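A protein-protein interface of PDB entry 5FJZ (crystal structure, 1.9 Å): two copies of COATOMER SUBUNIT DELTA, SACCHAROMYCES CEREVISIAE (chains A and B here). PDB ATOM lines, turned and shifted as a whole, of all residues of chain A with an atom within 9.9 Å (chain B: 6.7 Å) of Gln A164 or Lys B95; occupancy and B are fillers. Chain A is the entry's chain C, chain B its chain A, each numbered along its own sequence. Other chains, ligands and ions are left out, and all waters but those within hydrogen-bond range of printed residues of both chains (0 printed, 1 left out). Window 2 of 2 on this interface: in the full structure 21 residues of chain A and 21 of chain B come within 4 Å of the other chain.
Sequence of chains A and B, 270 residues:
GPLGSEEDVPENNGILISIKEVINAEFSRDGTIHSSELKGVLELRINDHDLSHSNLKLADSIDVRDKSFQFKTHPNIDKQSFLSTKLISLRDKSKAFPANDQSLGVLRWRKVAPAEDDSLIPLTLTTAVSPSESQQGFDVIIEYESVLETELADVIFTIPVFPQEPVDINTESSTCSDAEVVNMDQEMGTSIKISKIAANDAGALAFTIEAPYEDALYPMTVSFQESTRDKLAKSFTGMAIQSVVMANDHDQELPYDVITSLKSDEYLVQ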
ATOM      1  N   GLN A 135      -2.830  15.445  19.927  1.00  0.00           N
ATOM      2  CA  GLN A 135      -2.467  14.841  21.216  1.00  0.00           C
ATOM      3  C   GLN A 135      -3.258  15.575  22.286  1.00  0.00           C
ATOM      4  O   GLN A 135      -3.810  16.642  22.014  1.00  0.00           O
ATOM      5  CB  GLN A 135      -0.943  14.929  21.458  1.00  0.00           C
ATOM      6  CG  GLN A 135      -0.142  14.299  20.322  1.00  0.00           C
ATOM      7  CD  GLN A 135       1.326  14.004  20.613  1.00  0.00           C
ATOM      8  OE1 GLN A 135       2.112  13.698  19.692  1.00  0.00           O
ATOM      9  NE2 GLN A 135       1.713  14.081  21.891  1.00  0.00           N
ATOM     10  N   GLN A 136      -3.290  15.013  23.497  1.00  0.00           N
ATOM     11  CA  GLN A 136      -3.840  15.640  24.719  1.00  0.00           C
ATOM     12  C   GLN A 136      -2.775  16.568  25.313  1.00  0.00           C
ATOM     13  O   GLN A 136      -2.094  16.222  26.299  1.00  0.00           O
ATOM     14  CB  GLN A 136      -4.140  14.528  25.763  1.00  0.00           C
ATOM     15  CG  GLN A 136      -5.186  13.500  25.227  1.00  0.00           C
ATOM     16  CD  GLN A 136      -6.461  14.184  24.759  1.00  0.00           C
ATOM     17  OE1 GLN A 136      -7.041  14.960  25.524  1.00  0.00           O
ATOM     18  NE2 GLN A 136      -6.885  13.959  23.502  1.00  0.00           N
ATOM     19  N   VAL A 161       8.323  17.333  31.363  1.00  0.00           N
ATOM     20  CA  VAL A 161       7.165  16.477  31.366  1.00  0.00           C
ATOM     21  C   VAL A 161       7.726  15.146  30.918  1.00  0.00           C
ATOM     22  O   VAL A 161       8.748  15.082  30.191  1.00  0.00           O
ATOM     23  CB  VAL A 161       5.955  16.997  30.510  1.00  0.00           C
ATOM     24  CG1 VAL A 161       5.398  18.266  31.062  1.00  0.00           C
ATOM     25  CG2 VAL A 161       6.359  17.275  29.061  1.00  0.00           C
ATOM     26  N   PHE A 162       7.012  14.096  31.222  1.00  0.00           N
ATOM     27  CA  PHE A 162       7.335  12.779  30.709  1.00  0.00           C
ATOM     28  C   PHE A 162       6.099  12.136  30.063  1.00  0.00           C
ATOM     29  O   PHE A 162       5.393  11.430  30.719  1.00  0.00           O
ATOM     30  CB  PHE A 162       7.763  11.873  31.852  1.00  0.00           C
ATOM     31  CG  PHE A 162       9.004  12.326  32.528  1.00  0.00           C
ATOM     32  CD1 PHE A 162       8.935  13.297  33.464  1.00  0.00           C
ATOM     33  CD2 PHE A 162      10.215  11.725  32.271  1.00  0.00           C
ATOM     34  CE1 PHE A 162      10.071  13.718  34.102  1.00  0.00           C
ATOM     35  CE2 PHE A 162      11.377  12.163  32.875  1.00  0.00           C
ATOM     36  CZ  PHE A 162      11.293  13.130  33.844  1.00  0.00           C
ATOM     37  N   PRO A 163       5.859  12.370  28.752  1.00  0.00           N
ATOM     38  CA  PRO A 163       4.510  12.021  28.225  1.00  0.00           C
ATOM     39  C   PRO A 163       4.397  10.533  27.897  1.00  0.00           C
ATOM     40  O   PRO A 163       5.400   9.916  27.556  1.00  0.00           O
ATOM     41  CB  PRO A 163       4.382  12.902  26.977  1.00  0.00           C
ATOM     42  CG  PRO A 163       5.758  13.328  26.610  1.00  0.00           C
ATOM     43  CD  PRO A 163       6.586  13.280  27.864  1.00  0.00           C
ATOM     44  N   GLN A 164       3.186  10.006  28.028  1.00  0.00           N
ATOM     45  CA  GLN A 164       2.802   8.616  27.638  1.00  0.00           C
ATOM     46  C   GLN A 164       2.855   8.401  26.143  1.00  0.00           C
ATOM     47  O   GLN A 164       3.058   7.295  25.711  1.00  0.00           O
ATOM     48  CB  GLN A 164       1.351   8.324  28.077  1.00  0.00           C
ATOM     49  CG  GLN A 164       1.139   8.264  29.574  1.00  0.00           C
ATOM     50  CD  GLN A 164       1.711   7.000  30.204  1.00  0.00           C
ATOM     51  OE1 GLN A 164       1.238   5.879  29.961  1.00  0.00           O
ATOM     52  NE2 GLN A 164       2.707   7.176  31.062  1.00  0.00           N
ATOM     53  N   GLU A 165       2.600   9.457  25.361  1.00  0.00           N
ATOM     54  CA  GLU A 165       2.727   9.411  23.907  1.00  0.00           C
ATOM     55  C   GLU A 165       4.042  10.042  23.474  1.00  0.00           C
ATOM     56  O   GLU A 165       4.491  11.009  24.055  1.00  0.00           O
ATOM     57  CB  GLU A 165       1.559  10.214  23.308  1.00  0.00           C
ATOM     58  CG  GLU A 165       1.407  10.199  21.800  1.00  0.00           C
ATOM     59  CD  GLU A 165       0.917   8.866  21.252  1.00  0.00           C
ATOM     60  OE1 GLU A 165       0.454   8.005  22.038  1.00  0.00           O
ATOM     61  OE2 GLU A 165       1.049   8.672  20.028  1.00  0.00           O
ATOM     62  N   PRO A 166       4.651   9.540  22.414  1.00  0.00           N
ATOM     63  CA  PRO A 166       5.856  10.172  21.896  1.00  0.00           C
ATOM     64  C   PRO A 166       5.691  11.646  21.519  1.00  0.00           C
ATOM     65  O   PRO A 166       4.647  12.026  20.957  1.00  0.00           O
ATOM     66  CB  PRO A 166       6.154   9.398  20.604  1.00  0.00           C
ATOM     67  CG  PRO A 166       5.259   8.186  20.604  1.00  0.00           C
ATOM     68  CD  PRO A 166       4.327   8.261  21.758  1.00  0.00           C
ATOM     69  N   VAL A 167       6.757  12.435  21.679  1.00  0.00           N
ATOM     70  CA  VAL A 167       6.754  13.765  21.073  1.00  0.00           C
ATOM     71  C   VAL A 167       6.825  13.689  19.574  1.00  0.00           C
ATOM     72  O   VAL A 167       7.480  12.822  18.969  1.00  0.00           O
ATOM     73  CB  VAL A 167       7.681  14.855  21.688  1.00  0.00           C
ATOM     74  CG1 VAL A 167       8.670  14.322  22.664  1.00  0.00           C
ATOM     75  CG2 VAL A 167       8.359  15.669  20.592  1.00  0.00           C
ATOM     76  N   THR A 190      11.862  15.794  28.932  1.00  0.00           N
ATOM     77  CA  THR A 190      12.028  15.283  27.600  1.00  0.00           C
ATOM     78  C   THR A 190      12.879  16.248  26.816  1.00  0.00           C
ATOM     79  O   THR A 190      12.594  17.433  26.754  1.00  0.00           O
ATOM     80  CB  THR A 190      10.628  15.071  27.007  1.00  0.00           C
ATOM     81  OG1 THR A 190       9.881  14.152  27.808  1.00  0.00           O
ATOM     82  CG2 THR A 190      10.746  14.555  25.559  1.00  0.00           C
ATOM     83  N   ILE A 209       3.462  17.946  22.171  1.00  0.00           N
ATOM     84  CA  ILE A 209       3.835  17.132  23.359  1.00  0.00           C
ATOM     85  C   ILE A 209       2.659  17.132  24.359  1.00  0.00           C
ATOM     86  O   ILE A 209       1.975  18.125  24.473  1.00  0.00           O
ATOM     87  CB  ILE A 209       5.114  17.685  24.058  1.00  0.00           C
ATOM     88  CG1 ILE A 209       5.667  16.728  25.142  1.00  0.00           C
ATOM     89  CG2 ILE A 209       4.871  19.060  24.616  1.00  0.00           C
ATOM     90  CD1 ILE A 209       7.088  17.084  25.646  1.00  0.00           C
ATOM     91  N   GLU A 210       2.449  15.994  25.029  1.00  0.00           N
ATOM     92  CA  GLU A 210       1.431  15.858  26.013  1.00  0.00           C
ATOM     93  C   GLU A 210       1.789  16.460  27.313  1.00  0.00           C
ATOM     94  O   GLU A 210       2.892  16.275  27.765  1.00  0.00           O
ATOM     95  CB  GLU A 210       1.139  14.399  26.363  1.00  0.00           C
ATOM     96  CG  GLU A 210       0.354  13.626  25.373  1.00  0.00           C
ATOM     97  CD  GLU A 210      -0.007  12.211  25.866  1.00  0.00           C
ATOM     98  OE1 GLU A 210       0.561  11.750  26.897  1.00  0.00           O
ATOM     99  OE2 GLU A 210      -0.877  11.556  25.211  1.00  0.00           O
ATOM    100  N   ALA A 211       0.836  17.184  27.909  1.00  0.00           N
ATOM    101  CA  ALA A 211       0.992  17.801  29.212  1.00  0.00           C
ATOM    102  C   ALA A 211      -0.414  18.072  29.718  1.00  0.00           C
ATOM    103  O   ALA A 211      -1.323  18.276  28.912  1.00  0.00           O
ATOM    104  CB  ALA A 211       1.742  19.136  29.111  1.00  0.00           C
ATOM    105  N   PRO A 212      -0.579  18.152  31.033  1.00  0.00           N
ATOM    106  CA  PRO A 212      -1.911  18.280  31.592  1.00  0.00           C
ATOM    107  C   PRO A 212      -2.499  19.670  31.499  1.00  0.00           C
ATOM    108  O   PRO A 212      -3.717  19.801  31.489  1.00  0.00           O
ATOM    109  CB  PRO A 212      -1.727  17.826  33.055  1.00  0.00           C
ATOM    110  CG  PRO A 212      -0.266  17.860  33.330  1.00  0.00           C
ATOM    111  CD  PRO A 212       0.433  17.684  32.017  1.00  0.00           C
ATOM    112  N   HIS B  49       7.838   3.600  20.916  1.00  0.00           N
ATOM    113  CA  HIS B  49       6.554   3.508  21.566  1.00  0.00           C
ATOM    114  C   HIS B  49       5.978   2.058  21.623  1.00  0.00           C
ATOM    115  O   HIS B  49       5.255   1.699  22.515  1.00  0.00           O
ATOM    116  CB  HIS B  49       5.560   4.481  20.877  1.00  0.00           C
ATOM    117  CG  HIS B  49       6.052   5.156  19.602  1.00  0.00           C
ATOM    118  ND1 HIS B  49       7.152   6.006  19.540  1.00  0.00           N
ATOM    119  CD2 HIS B  49       5.504   5.174  18.363  1.00  0.00           C
ATOM    120  CE1 HIS B  49       7.271   6.481  18.312  1.00  0.00           C
ATOM    121  NE2 HIS B  49       6.284   5.990  17.578  1.00  0.00           N
ATOM    122  N   SER B  52       6.965   0.265  24.920  1.00  0.00           N
ATOM    123  CA  SER B  52       6.776   1.024  26.104  1.00  0.00           C
ATOM    124  C   SER B  52       5.873   0.309  27.088  1.00  0.00           C
ATOM    125  O   SER B  52       5.864   0.664  28.247  1.00  0.00           O
ATOM    126  CB  SER B  52       6.192   2.424  25.789  1.00  0.00           C
ATOM    127  OG  SER B  52       4.867   2.338  25.304  1.00  0.00           O
ATOM    128  N   HIS B  53       5.133  -0.698  26.628  1.00  0.00           N
ATOM    129  CA  HIS B  53       4.245  -1.491  27.523  1.00  0.00           C
ATOM    130  C   HIS B  53       4.939  -2.777  27.899  1.00  0.00           C
ATOM    131  O   HIS B  53       4.491  -3.863  27.547  1.00  0.00           O
ATOM    132  CB  HIS B  53       2.937  -1.817  26.786  1.00  0.00           C
ATOM    133  CG  HIS B  53       1.995  -0.660  26.684  1.00  0.00           C
ATOM    134  ND1 HIS B  53       1.994   0.201  25.604  1.00  0.00           N
ATOM    135  CD2 HIS B  53       1.027  -0.222  27.521  1.00  0.00           C
ATOM    136  CE1 HIS B  53       1.070   1.130  25.784  1.00  0.00           C
ATOM    137  NE2 HIS B  53       0.450   0.883  26.927  1.00  0.00           N
ATOM    138  N   LEU B  90       4.852  -1.365  36.084  1.00  0.00           N
ATOM    139  CA  LEU B  90       4.176  -0.176  36.658  1.00  0.00           C
ATOM    140  C   LEU B  90       3.118  -0.513  37.701  1.00  0.00           C
ATOM    141  O   LEU B  90       2.443  -1.517  37.591  1.00  0.00           O
ATOM    142  CB  LEU B  90       3.584   0.674  35.527  1.00  0.00           C
ATOM    143  CG  LEU B  90       4.662   1.306  34.651  1.00  0.00           C
ATOM    144  CD1 LEU B  90       4.050   1.870  33.397  1.00  0.00           C
ATOM    145  CD2 LEU B  90       5.394   2.407  35.396  1.00  0.00           C
ATOM    146  N   ASP B  92       0.480   1.349  38.230  1.00  0.00           N
ATOM    147  CA  ASP B  92      -0.789   1.555  37.453  1.00  0.00           C
ATOM    148  C   ASP B  92      -0.755   0.771  36.175  1.00  0.00           C
ATOM    149  O   ASP B  92      -0.056   1.135  35.231  1.00  0.00           O
ATOM    150  CB  ASP B  92      -0.953   3.048  37.136  1.00  0.00           C
ATOM    151  CG  ASP B  92      -2.286   3.386  36.458  1.00  0.00           C
ATOM    152  OD1 ASP B  92      -2.916   2.551  35.754  1.00  0.00           O
ATOM    153  OD2 ASP B  92      -2.666   4.567  36.601  1.00  0.00           O
ATOM    154  N   LYS B  93      -1.509  -0.331  36.105  1.00  0.00           N
ATOM    155  CA  LYS B  93      -1.342  -1.299  34.978  1.00  0.00           C
ATOM    156  C   LYS B  93      -1.905  -0.742  33.650  1.00  0.00           C
ATOM    157  O   LYS B  93      -1.646  -1.264  32.592  1.00  0.00           O
ATOM    158  CB  LYS B  93      -2.004  -2.637  35.327  1.00  0.00           C
ATOM    159  CG  LYS B  93      -1.571  -3.255  36.669  1.00  0.00           C
ATOM    160  CD  LYS B  93      -0.067  -3.527  36.784  1.00  0.00           C
ATOM    161  CE  LYS B  93       0.417  -4.611  35.809  1.00  0.00           C
ATOM    162  NZ  LYS B  93       1.549  -5.462  36.307  1.00  0.00           N
ATOM    163  N   SER B  94      -2.673   0.344  33.700  1.00  0.00           N
ATOM    164  CA  SER B  94      -3.106   0.929  32.455  1.00  0.00           C
ATOM    165  C   SER B  94      -2.052   1.863  31.829  1.00  0.00           C
ATOM    166  O   SER B  94      -2.274   2.333  30.752  1.00  0.00           O
ATOM    167  CB  SER B  94      -4.388   1.750  32.646  1.00  0.00           C
ATOM    168  OG  SER B  94      -4.111   3.016  33.192  1.00  0.00           O
ATOM    169  N   LYS B  95      -0.951   2.187  32.511  1.00  0.00           N
ATOM    170  CA  LYS B  95      -0.010   3.140  31.929  1.00  0.00           C
ATOM    171  C   LYS B  95       1.140   2.452  31.263  1.00  0.00           C
ATOM    172  O   LYS B  95       1.251   1.257  31.341  1.00  0.00           O
ATOM    173  CB  LYS B  95       0.458   4.093  33.022  1.00  0.00           C
ATOM    174  CG  LYS B  95      -0.370   5.363  33.035  1.00  0.00           C
ATOM    175  CD  LYS B  95      -0.834   5.686  34.432  1.00  0.00           C
ATOM    176  CE  LYS B  95      -1.554   7.034  34.486  1.00  0.00           C
ATOM    177  NZ  LYS B  95      -2.867   7.026  33.784  1.00  0.00           N
ATOM    178  N   ALA B  96       1.999   3.209  30.594  1.00  0.00           N
ATOM    179  CA  ALA B  96       3.164   2.640  29.926  1.00  0.00           C
ATOM    180  C   ALA B  96       4.360   3.482  30.300  1.00  0.00           C
ATOM    181  O   ALA B  96       4.205   4.576  30.879  1.00  0.00           O
ATOM    182  CB  ALA B  96       2.991   2.688  28.443  1.00  0.00           C
ATOM    183  N   PHE B  97       5.561   2.995  30.004  1.00  0.00           N
ATOM    184  CA  PHE B  97       6.740   3.780  30.332  1.00  0.00           C
ATOM    185  C   PHE B  97       6.898   4.940  29.392  1.00  0.00           C
ATOM    186  O   PHE B  97       6.729   4.799  28.176  1.00  0.00           O
ATOM    187  CB  PHE B  97       8.019   2.920  30.253  1.00  0.00           C
ATOM    188  CG  PHE B  97       8.181   1.974  31.410  1.00  0.00           C
ATOM    189  CD1 PHE B  97       8.501   2.442  32.639  1.00  0.00           C
ATOM    190  CD2 PHE B  97       8.018   0.637  31.233  1.00  0.00           C
ATOM    191  CE1 PHE B  97       8.654   1.599  33.727  1.00  0.00           C
ATOM    192  CE2 PHE B  97       8.180  -0.226  32.288  1.00  0.00           C
ATOM    193  CZ  PHE B  97       8.551   0.243  33.514  1.00  0.00           C
ATOM    194  N   PRO B  98       7.238   6.104  29.909  1.00  0.00           N
ATOM    195  CA  PRO B  98       7.684   7.101  28.953  1.00  0.00           C
ATOM    196  C   PRO B  98       8.688   6.602  27.921  1.00  0.00           C
ATOM    197  O   PRO B  98       9.683   5.994  28.277  1.00  0.00           O
ATOM    198  CB  PRO B  98       8.330   8.202  29.875  1.00  0.00           C
ATOM    199  CG  PRO B  98       7.672   8.006  31.148  1.00  0.00           C
ATOM    200  CD  PRO B  98       7.450   6.535  31.283  1.00  0.00           C
ATOM    201  N   ALA B  99       8.439   6.924  26.653  1.00  0.00           N
ATOM    202  CA  ALA B  99       9.147   6.397  25.538  1.00  0.00           C
ATOM    203  C   ALA B  99       9.759   7.465  24.670  1.00  0.00           C
ATOM    204  O   ALA B  99       9.922   7.261  23.480  1.00  0.00           O
ATOM    205  CB  ALA B  99       8.193   5.484  24.732  1.00  0.00           C
ATOM    206  N   ASN B 100      10.216   8.561  25.286  1.00  0.00           N
ATOM    207  CA  ASN B 100      11.065   9.539  24.607  1.00  0.00           C
ATOM    208  C   ASN B 100      12.524   9.566  25.124  1.00  0.00           C
ATOM    209  O   ASN B 100      13.126  10.645  25.285  1.00  0.00           O
ATOM    210  CB  ASN B 100      10.426  10.912  24.684  1.00  0.00           C
ATOM    211  CG  ASN B 100       9.124  11.012  23.880  1.00  0.00           C
ATOM    212  OD1 ASN B 100       9.123  10.998  22.678  1.00  0.00           O
ATOM    213  ND2 ASN B 100       8.025  11.124  24.567  1.00  0.00           N
ATOM    214  N   ALA B 247       4.074  -6.434  28.836  1.00  0.00           N
ATOM    215  CA  ALA B 247       3.475  -6.370  30.142  1.00  0.00           C
ATOM    216  C   ALA B 247       2.243  -7.254  30.197  1.00  0.00           C
ATOM    217  O   ALA B 247       1.926  -7.800  31.242  1.00  0.00           O
ATOM    218  CB  ALA B 247       3.101  -4.951  30.539  1.00  0.00           C
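No position is printed for both chains. Of the 10 pairs that touch across the chains among the printed residues, none has its exchanged pair printed and touching as well.
Along chain B the printed residues that touch a printed residue of chain A span positions 49 to 100. Hydrophobic or aromatic side chains of chain A within 4 Å of the printed part of chain B: Phe A162, Pro A163, Pro A166 and Val A167. Among the printed residues, 10 pairs touch across the chains.
Gln A164 touches two residues of chain B. Printed residues of chain A within 4 Å of Lys B95: Gln A164 (3.5 Å). No residue of chain A comes within 4 Å of Ser B94. Printed residues of chain A within 4 Å of Asn B100: Pro A163 (3.8 Å), Glu A165 (3.6 Å), Pro A166 (3.5 Å), Val A167 (2.9 Å) and Thr A190 (3.8 Å). Printed residues of chain B within 4 Å of Thr A190: Asn B100 (3.8 Å). Of the printed residues of chain B, Val A167 touches Asn B100 (2.9 Å). Of the printed residues of chain A, His B49 touches Pro A166 (3.1 Å). Ala B99 touches none of the printed residues of chain A. Gln A135 touches none of the printed residues of chain B. The nearest printed residue of chain B that does not touch Gln A164 is Pro B98 (4.8 Å). The nearest printed residue of chain A that does not touch Lys B95 is Phe A162 (8.7 Å). The nearest printed residue of chain B that does not touch Phe A162 is Asn B100 (5.9 Å).
Pro B98 touches Phe A162 (CG to CB, 3.9 Å). Pro A163 touches Pro B98 (O to CA, 3.9 Å). Asn B100 touches Pro A163. OE1 of Gln A164 touches CG of Lys B95, at 3.5 Å. Glu A165 touches Asn B100. ND1 of His B49 touches CG of Pro A166, 3.1 Å away. CA of Pro A166 touches OD1 of Asn B100, 3.5 Å away. CB of Asn B100 touches CG2 of Thr A190, 3.8 Å away.
O of His B49 lies within hydrogen-bond range of OG of Ser B52, at 2.9 Å. The side-chain amino group (NZ) of Lys B95 lies within salt-bridge range of the side-chain carboxylate (OD2) of Asp B92, 3.7 Å away. OE1 of Gln A135 sits close to O of Pro A166 (3.3 Å). The side-chain hydroxyl (OG1) of Thr A190 sits at hydrogen-bond distance from the backbone carbonyl oxygen (O) of Val A161 (2.8 Å). N of Gln A164 lies within hydrogen-bond range of OE1 of Glu A210, 3.3 Å away. N of Glu A165 is in hydrogen-bond range of OE1 of Glu A210, at 3.4 Å.
OE1 of Gln A164 is in hydrogen-bond range of N of Ala B96, 2.8 Å away. The side-chain amide oxygen (OD1) of Asn B100 sits at hydrogen-bond distance from the backbone NH (N) of Val A167 (2.9 Å).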
